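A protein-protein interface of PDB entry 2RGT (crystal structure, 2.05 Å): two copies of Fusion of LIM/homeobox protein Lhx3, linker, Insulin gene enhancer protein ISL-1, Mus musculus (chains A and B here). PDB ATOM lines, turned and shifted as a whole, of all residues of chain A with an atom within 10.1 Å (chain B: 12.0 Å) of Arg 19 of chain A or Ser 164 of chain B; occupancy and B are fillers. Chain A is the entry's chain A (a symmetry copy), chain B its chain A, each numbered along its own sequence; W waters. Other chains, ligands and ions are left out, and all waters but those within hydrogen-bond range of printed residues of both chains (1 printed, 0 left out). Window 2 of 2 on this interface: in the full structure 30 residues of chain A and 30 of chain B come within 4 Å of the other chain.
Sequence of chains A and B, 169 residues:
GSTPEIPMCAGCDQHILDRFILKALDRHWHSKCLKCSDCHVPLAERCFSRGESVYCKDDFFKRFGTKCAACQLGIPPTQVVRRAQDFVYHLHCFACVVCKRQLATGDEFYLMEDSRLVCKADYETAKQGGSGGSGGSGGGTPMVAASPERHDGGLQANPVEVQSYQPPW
No residue of chain B comes within 4 Å of Asp 18 of chain A. Arg 19 of chain A touches one residue of chain B. Phe 20 of chain A touches just these residues of chain B: Gln 163 and Ser 164. Ile 21 of chain A touches just these residues of chain B: Glu 161 (3.9 Å), Val 162 (3.4 Å) and Gln 163 (2.6 Å). Printed residues of chain B within 4 Å of Lys 23 of chain A: Val 160 (3.5 Å), Glu 161 (2.5 Å) and Gln 163 (3.3 Å). Of the printed residues of chain A, Val 162 of chain B touches Ile 21 and Leu 22. Printed residues of chain A within 4 Å of Gln 163 of chain B: Phe 20, Ile 21, Lys 23 and His 28. Of chain A, only Arg 19 and Phe 20 come within 4 Å of Ser 164 of chain B. The nearest residue of chain B that does not touch Arg 19 of chain A is Gln 163 of chain B (4.2 Å). The nearest printed residue of chain A that does not touch Glu 161 of chain B is Trp 29 of chain A (7.0 Å).
The backbone NH of Leu 22 of chain A is in hydrogen-bond range of the backbone carbonyl oxygen of Trp 29 of chain A, at 3.1 Å.
O of Glu 161 of chain B sits at hydrogen-bond distance from N of Lys 23 of chain A. O of Gln 163 of chain B lies within hydrogen-bond range of N of Ile 21 of chain A, at 2.6 Å.
No position is printed for both chains. Of the 13 pairs that touch across the chains among the printed residues, none has its exchanged pair printed and touching as well.
Water W1 bridges the side-chain carboxylate of Glu 161 of chain B (2.9 Å) and the backbone carbonyl oxygen of Lys 23 of chain A (2.9 Å).
Along chain B the printed residues that touch a printed residue of chain A span positions 160 to 164.
O of Arg 19 of chain A touches CA of Ser 164 of chain B, 3.4 Å away. Phe 20 of chain A touches Gln 163 of chain B (C to O, 3.6 Å). Phe 20 of chain A touches Ser 164 of chain B (CD1 to CB, 3.9 Å). O of Ile 21 of chain A touches O of Glu 161 of chain B, at 3.9 Å. O of Ile 21 of chain A touches CA of Val 162 of chain B, 3.4 Å away. Val 160 of chain B touches Leu 22 of chain A (CG1 to CD1, 3.8 Å). O of Glu 161 of chain B touches C of Leu 22 of chain A, 3.3 Å away. O of Lys 23 of chain A touches CA of Val 160 of chain B (3.5 Å). CB of Lys 23 of chain A touches NE2 of Gln 163 of chain B (3.3 Å). His 28 of chain A touches Gln 163 of chain B (NE2 to OE1, 3.7 Å).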
ATOM      1  N   PRO A   7     -21.434  23.086 -30.976  1.00  0.00           N
ATOM      2  CA  PRO A   7     -21.370  22.963 -29.500  1.00  0.00           C
ATOM      3  C   PRO A   7     -20.151  22.147 -29.024  1.00  0.00           C
ATOM      4  O   PRO A   7     -20.201  20.919 -29.009  1.00  0.00           O
ATOM      5  CB  PRO A   7     -22.677  22.247 -29.163  1.00  0.00           C
ATOM      6  CG  PRO A   7     -23.636  22.721 -30.213  1.00  0.00           C
ATOM      7  CD  PRO A   7     -22.820  23.026 -31.474  1.00  0.00           C
ATOM      8  N   HIS A  15     -17.143  17.850 -29.911  1.00  0.00           N
ATOM      9  CA  HIS A  15     -18.442  18.536 -29.950  1.00  0.00           C
ATOM     10  C   HIS A  15     -19.631  17.635 -29.580  1.00  0.00           C
ATOM     11  O   HIS A  15     -19.467  16.426 -29.417  1.00  0.00           O
ATOM     12  CB  HIS A  15     -18.673  19.172 -31.322  1.00  0.00           C
ATOM     13  CG  HIS A  15     -17.594  20.126 -31.735  1.00  0.00           C
ATOM     14  ND1 HIS A  15     -16.362  19.705 -32.186  1.00  0.00           N
ATOM     15  CD2 HIS A  15     -17.564  21.478 -31.763  1.00  0.00           C
ATOM     16  CE1 HIS A  15     -15.619  20.759 -32.475  1.00  0.00           C
ATOM     17  NE2 HIS A  15     -16.324  21.847 -32.228  1.00  0.00           N
ATOM     18  N   ILE A  16     -20.823  18.224 -29.448  1.00  0.00           N
ATOM     19  CA  ILE A  16     -21.956  17.536 -28.759  1.00  0.00           C
ATOM     20  C   ILE A  16     -23.192  17.320 -29.631  1.00  0.00           C
ATOM     21  O   ILE A  16     -23.874  18.274 -30.000  1.00  0.00           O
ATOM     22  CB  ILE A  16     -22.409  18.269 -27.458  1.00  0.00           C
ATOM     23  CG1 ILE A  16     -21.209  18.725 -26.632  1.00  0.00           C
ATOM     24  CG2 ILE A  16     -23.315  17.379 -26.611  1.00  0.00           C
ATOM     25  CD1 ILE A  16     -21.519  19.892 -25.728  1.00  0.00           C
ATOM     26  N   LEU A  17     -23.487  16.054 -29.916  1.00  0.00           N
ATOM     27  CA  LEU A  17     -24.637  15.674 -30.744  1.00  0.00           C
ATOM     28  C   LEU A  17     -25.859  15.196 -29.957  1.00  0.00           C
ATOM     29  O   LEU A  17     -26.974  15.190 -30.482  1.00  0.00           O
ATOM     30  CB  LEU A  17     -24.222  14.606 -31.766  1.00  0.00           C
ATOM     31  CG  LEU A  17     -24.184  14.952 -33.257  1.00  0.00           C
ATOM     32  CD1 LEU A  17     -23.478  16.274 -33.519  1.00  0.00           C
ATOM     33  CD2 LEU A  17     -23.520  13.799 -34.006  1.00  0.00           C
ATOM     34  N   ASP A  18     -25.642  14.809 -28.701  1.00  0.00           N
ATOM     35  CA  ASP A  18     -26.673  14.202 -27.838  1.00  0.00           C
ATOM     36  C   ASP A  18     -28.049  14.885 -27.845  1.00  0.00           C
ATOM     37  O   ASP A  18     -28.171  16.111 -28.066  1.00  0.00           O
ATOM     38  CB  ASP A  18     -26.169  14.051 -26.383  1.00  0.00           C
ATOM     39  CG  ASP A  18     -24.863  13.255 -26.280  1.00  0.00           C
ATOM     40  OD1 ASP A  18     -24.326  12.761 -27.312  1.00  0.00           O
ATOM     41  OD2 ASP A  18     -24.352  13.146 -25.148  1.00  0.00           O
ATOM     42  N   ARG A  19     -29.073  14.057 -27.611  1.00  0.00           N
ATOM     43  CA  ARG A  19     -30.449  14.509 -27.387  1.00  0.00           C
ATOM     44  C   ARG A  19     -30.509  15.666 -26.373  1.00  0.00           C
ATOM     45  O   ARG A  19     -31.158  16.688 -26.624  1.00  0.00           O
ATOM     46  CB  ARG A  19     -31.321  13.341 -26.893  1.00  0.00           C
ATOM     47  CG  ARG A  19     -32.167  12.747 -27.817  1.00  0.00           C
ATOM     48  CD  ARG A  19     -32.884  11.536 -27.219  1.00  0.00           C
ATOM     49  NE  ARG A  19     -32.130  10.303 -27.424  1.00  0.00           N
ATOM     50  CZ  ARG A  19     -32.585   9.233 -28.069  1.00  0.00           C
ATOM     51  NH1 ARG A  19     -33.808   9.222 -28.592  1.00  0.00           N
ATOM     52  NH2 ARG A  19     -31.808   8.167 -28.191  1.00  0.00           N
ATOM     53  N   PHE A  20     -29.802  15.511 -25.254  1.00  0.00           N
ATOM     54  CA  PHE A  20     -29.803  16.531 -24.211  1.00  0.00           C
ATOM     55  C   PHE A  20     -28.437  17.099 -23.969  1.00  0.00           C
ATOM     56  O   PHE A  20     -27.465  16.348 -23.910  1.00  0.00           O
ATOM     57  CB  PHE A  20     -30.360  15.955 -22.932  1.00  0.00           C
ATOM     58  CG  PHE A  20     -31.683  15.298 -23.114  1.00  0.00           C
ATOM     59  CD1 PHE A  20     -32.841  16.067 -23.181  1.00  0.00           C
ATOM     60  CD2 PHE A  20     -31.770  13.913 -23.243  1.00  0.00           C
ATOM     61  CE1 PHE A  20     -34.071  15.465 -23.365  1.00  0.00           C
ATOM     62  CE2 PHE A  20     -32.983  13.291 -23.419  1.00  0.00           C
ATOM     63  CZ  PHE A  20     -34.143  14.067 -23.486  1.00  0.00           C
ATOM     64  N   ILE A  21     -28.382  18.429 -23.840  1.00  0.00           N
ATOM     65  CA  ILE A  21     -27.138  19.199 -23.669  1.00  0.00           C
ATOM     66  C   ILE A  21     -27.160  19.856 -22.291  1.00  0.00           C
ATOM     67  O   ILE A  21     -28.193  20.380 -21.882  1.00  0.00           O
ATOM     68  CB  ILE A  21     -26.992  20.332 -24.766  1.00  0.00           C
ATOM     69  CG1 ILE A  21     -27.369  19.823 -26.159  1.00  0.00           C
ATOM     70  CG2 ILE A  21     -25.579  20.938 -24.772  1.00  0.00           C
ATOM     71  CD1 ILE A  21     -26.243  19.220 -26.905  1.00  0.00           C
ATOM     72  N   LEU A  22     -26.027  19.827 -21.596  1.00  0.00           N
ATOM     73  CA  LEU A  22     -25.895  20.499 -20.309  1.00  0.00           C
ATOM     74  C   LEU A  22     -25.298  21.893 -20.465  1.00  0.00           C
ATOM     75  O   LEU A  22     -24.359  22.096 -21.235  1.00  0.00           O
ATOM     76  CB  LEU A  22     -25.041  19.665 -19.353  1.00  0.00           C
ATOM     77  CG  LEU A  22     -25.715  18.440 -18.733  1.00  0.00           C
ATOM     78  CD1 LEU A  22     -24.953  17.970 -17.504  1.00  0.00           C
ATOM     79  CD2 LEU A  22     -27.165  18.743 -18.385  1.00  0.00           C
ATOM     80  N   LYS A  23     -25.851  22.852 -19.729  1.00  0.00           N
ATOM     81  CA  LYS A  23     -25.257  24.182 -19.614  1.00  0.00           C
ATOM     82  C   LYS A  23     -24.734  24.413 -18.187  1.00  0.00           C
ATOM     83  O   LYS A  23     -25.500  24.351 -17.219  1.00  0.00           O
ATOM     84  CB  LYS A  23     -26.292  25.253 -19.998  1.00  0.00           C
ATOM     85  CG  LYS A  23     -25.831  26.246 -21.103  1.00  0.00           C
ATOM     86  CD  LYS A  23     -25.165  27.544 -20.561  1.00  0.00           C
ATOM     87  CE  LYS A  23     -24.109  28.090 -21.560  1.00  0.00           C
ATOM     88  NZ  LYS A  23     -23.933  29.580 -21.578  1.00  0.00           N
ATOM     89  N   HIS A  28     -20.580  24.137 -22.406  1.00  0.00           N
ATOM     90  CA  HIS A  28     -21.474  23.136 -22.976  1.00  0.00           C
ATOM     91  C   HIS A  28     -20.889  21.734 -22.843  1.00  0.00           C
ATOM     92  O   HIS A  28     -19.733  21.498 -23.193  1.00  0.00           O
ATOM     93  CB  HIS A  28     -21.761  23.448 -24.445  1.00  0.00           C
ATOM     94  CG  HIS A  28     -22.936  24.353 -24.653  1.00  0.00           C
ATOM     95  ND1 HIS A  28     -22.833  25.574 -25.283  1.00  0.00           N
ATOM     96  CD2 HIS A  28     -24.240  24.214 -24.313  1.00  0.00           C
ATOM     97  CE1 HIS A  28     -24.023  26.149 -25.322  1.00  0.00           C
ATOM     98  NE2 HIS A  28     -24.894  25.344 -24.741  1.00  0.00           N
ATOM     99  N   TRP A  29     -21.695  20.808 -22.334  1.00  0.00           N
ATOM    100  CA  TRP A  29     -21.195  19.498 -21.920  1.00  0.00           C
ATOM    101  C   TRP A  29     -22.075  18.351 -22.443  1.00  0.00           C
ATOM    102  O   TRP A  29     -23.312  18.460 -22.414  1.00  0.00           O
ATOM    103  CB  TRP A  29     -21.175  19.396 -20.367  1.00  0.00           C
ATOM    104  CG  TRP A  29     -20.497  20.532 -19.635  1.00  0.00           C
ATOM    105  CD1 TRP A  29     -21.022  21.768 -19.353  1.00  0.00           C
ATOM    106  CD2 TRP A  29     -19.174  20.526 -19.093  1.00  0.00           C
ATOM    107  NE1 TRP A  29     -20.095  22.537 -18.692  1.00  0.00           N
ATOM    108  CE2 TRP A  29     -18.949  21.804 -18.524  1.00  0.00           C
ATOM    109  CE3 TRP A  29     -18.148  19.565 -19.042  1.00  0.00           C
ATOM    110  CZ2 TRP A  29     -17.749  22.138 -17.869  1.00  0.00           C
ATOM    111  CZ3 TRP A  29     -16.931  19.906 -18.414  1.00  0.00           C
ATOM    112  CH2 TRP A  29     -16.756  21.179 -17.820  1.00  0.00           C
ATOM    113  N   HIS A  30     -21.446  17.251 -22.877  1.00  0.00           N
ATOM    114  CA  HIS A  30     -22.102  15.935 -22.807  1.00  0.00           C
ATOM    115  C   HIS A  30     -22.379  15.722 -21.330  1.00  0.00           C
ATOM    116  O   HIS A  30     -21.559  16.118 -20.506  1.00  0.00           O
ATOM    117  CB  HIS A  30     -21.173  14.790 -23.215  1.00  0.00           C
ATOM    118  CG  HIS A  30     -20.682  14.860 -24.625  1.00  0.00           C
ATOM    119  ND1 HIS A  30     -19.372  15.157 -24.938  1.00  0.00           N
ATOM    120  CD2 HIS A  30     -21.324  14.679 -25.802  1.00  0.00           C
ATOM    121  CE1 HIS A  30     -19.234  15.160 -26.251  1.00  0.00           C
ATOM    122  NE2 HIS A  30     -20.403  14.877 -26.796  1.00  0.00           N
ATOM    123  N   SER A  31     -23.484  15.061 -20.984  1.00  0.00           N
ATOM    124  CA  SER A  31     -23.788  14.767 -19.569  1.00  0.00           C
ATOM    125  C   SER A  31     -22.850  13.712 -18.920  1.00  0.00           C
ATOM    126  O   SER A  31     -22.695  13.672 -17.692  1.00  0.00           O
ATOM    127  CB  SER A  31     -25.276  14.429 -19.382  1.00  0.00           C
ATOM    128  OG  SER A  31     -25.649  13.227 -20.029  1.00  0.00           O
ATOM    129  N   VAL B 160     -26.578  23.777 -13.047  1.00  0.00           N
ATOM    130  CA  VAL B 160     -26.479  22.874 -14.188  1.00  0.00           C
ATOM    131  C   VAL B 160     -27.824  22.886 -14.946  1.00  0.00           C
ATOM    132  O   VAL B 160     -28.776  22.185 -14.548  1.00  0.00           O
ATOM    133  CB  VAL B 160     -26.162  21.412 -13.729  1.00  0.00           C
ATOM    134  CG1 VAL B 160     -26.167  20.451 -14.903  1.00  0.00           C
ATOM    135  CG2 VAL B 160     -24.845  21.360 -12.993  1.00  0.00           C
ATOM    136  N   GLU B 161     -27.892  23.672 -16.028  1.00  0.00           N
ATOM    137  CA  GLU B 161     -29.080  23.738 -16.893  1.00  0.00           C
ATOM    138  C   GLU B 161     -29.051  22.777 -18.066  1.00  0.00           C
ATOM    139  O   GLU B 161     -27.988  22.448 -18.596  1.00  0.00           O
ATOM    140  CB  GLU B 161     -29.282  25.153 -17.411  1.00  0.00           C
ATOM    141  CG  GLU B 161     -30.011  26.048 -16.443  1.00  0.00           C
ATOM    142  CD  GLU B 161     -29.553  27.496 -16.518  1.00  0.00           C
ATOM    143  OE1 GLU B 161     -28.760  27.850 -17.434  1.00  0.00           O
ATOM    144  OE2 GLU B 161     -29.989  28.287 -15.644  1.00  0.00           O
ATOM    145  N   VAL B 162     -30.248  22.361 -18.475  1.00  0.00           N
ATOM    146  CA  VAL B 162     -30.467  21.374 -19.532  1.00  0.00           C
ATOM    147  C   VAL B 162     -31.131  21.992 -20.792  1.00  0.00           C
ATOM    148  O   VAL B 162     -32.130  22.717 -20.669  1.00  0.00           O
ATOM    149  CB  VAL B 162     -31.363  20.243 -19.025  1.00  0.00           C
ATOM    150  CG1 VAL B 162     -31.456  19.130 -20.068  1.00  0.00           C
ATOM    151  CG2 VAL B 162     -30.859  19.706 -17.686  1.00  0.00           C
ATOM    152  N   GLN B 163     -30.590  21.655 -21.966  1.00  0.00           N
ATOM    153  CA  GLN B 163     -31.122  22.055 -23.281  1.00  0.00           C
ATOM    154  C   GLN B 163     -31.264  20.855 -24.208  1.00  0.00           C
ATOM    155  O   GLN B 163     -30.300  20.132 -24.430  1.00  0.00           O
ATOM    156  CB  GLN B 163     -30.154  23.020 -23.962  1.00  0.00           C
ATOM    157  CG  GLN B 163     -30.370  24.469 -23.645  1.00  0.00           C
ATOM    158  CD  GLN B 163     -29.197  25.073 -22.929  1.00  0.00           C
ATOM    159  OE1 GLN B 163     -28.374  25.754 -23.529  1.00  0.00           O
ATOM    160  NE2 GLN B 163     -29.115  24.829 -21.634  1.00  0.00           N
ATOM    161  N   SER B 164     -32.444  20.665 -24.787  1.00  0.00           N
ATOM    162  CA  SER B 164     -32.640  19.591 -25.768  1.00  0.00           C
ATOM    163  C   SER B 164     -32.401  20.073 -27.205  1.00  0.00           C
ATOM    164  O   SER B 164     -31.274  20.430 -27.575  1.00  0.00           O
ATOM    165  CB  SER B 164     -34.016  18.928 -25.618  1.00  0.00           C
ATOM    166  OG  SER B 164     -35.033  19.901 -25.527  1.00  0.00           O
HETATM  167  O   HOH W   1     -26.105  27.137 -16.577  1.00  0.00           O
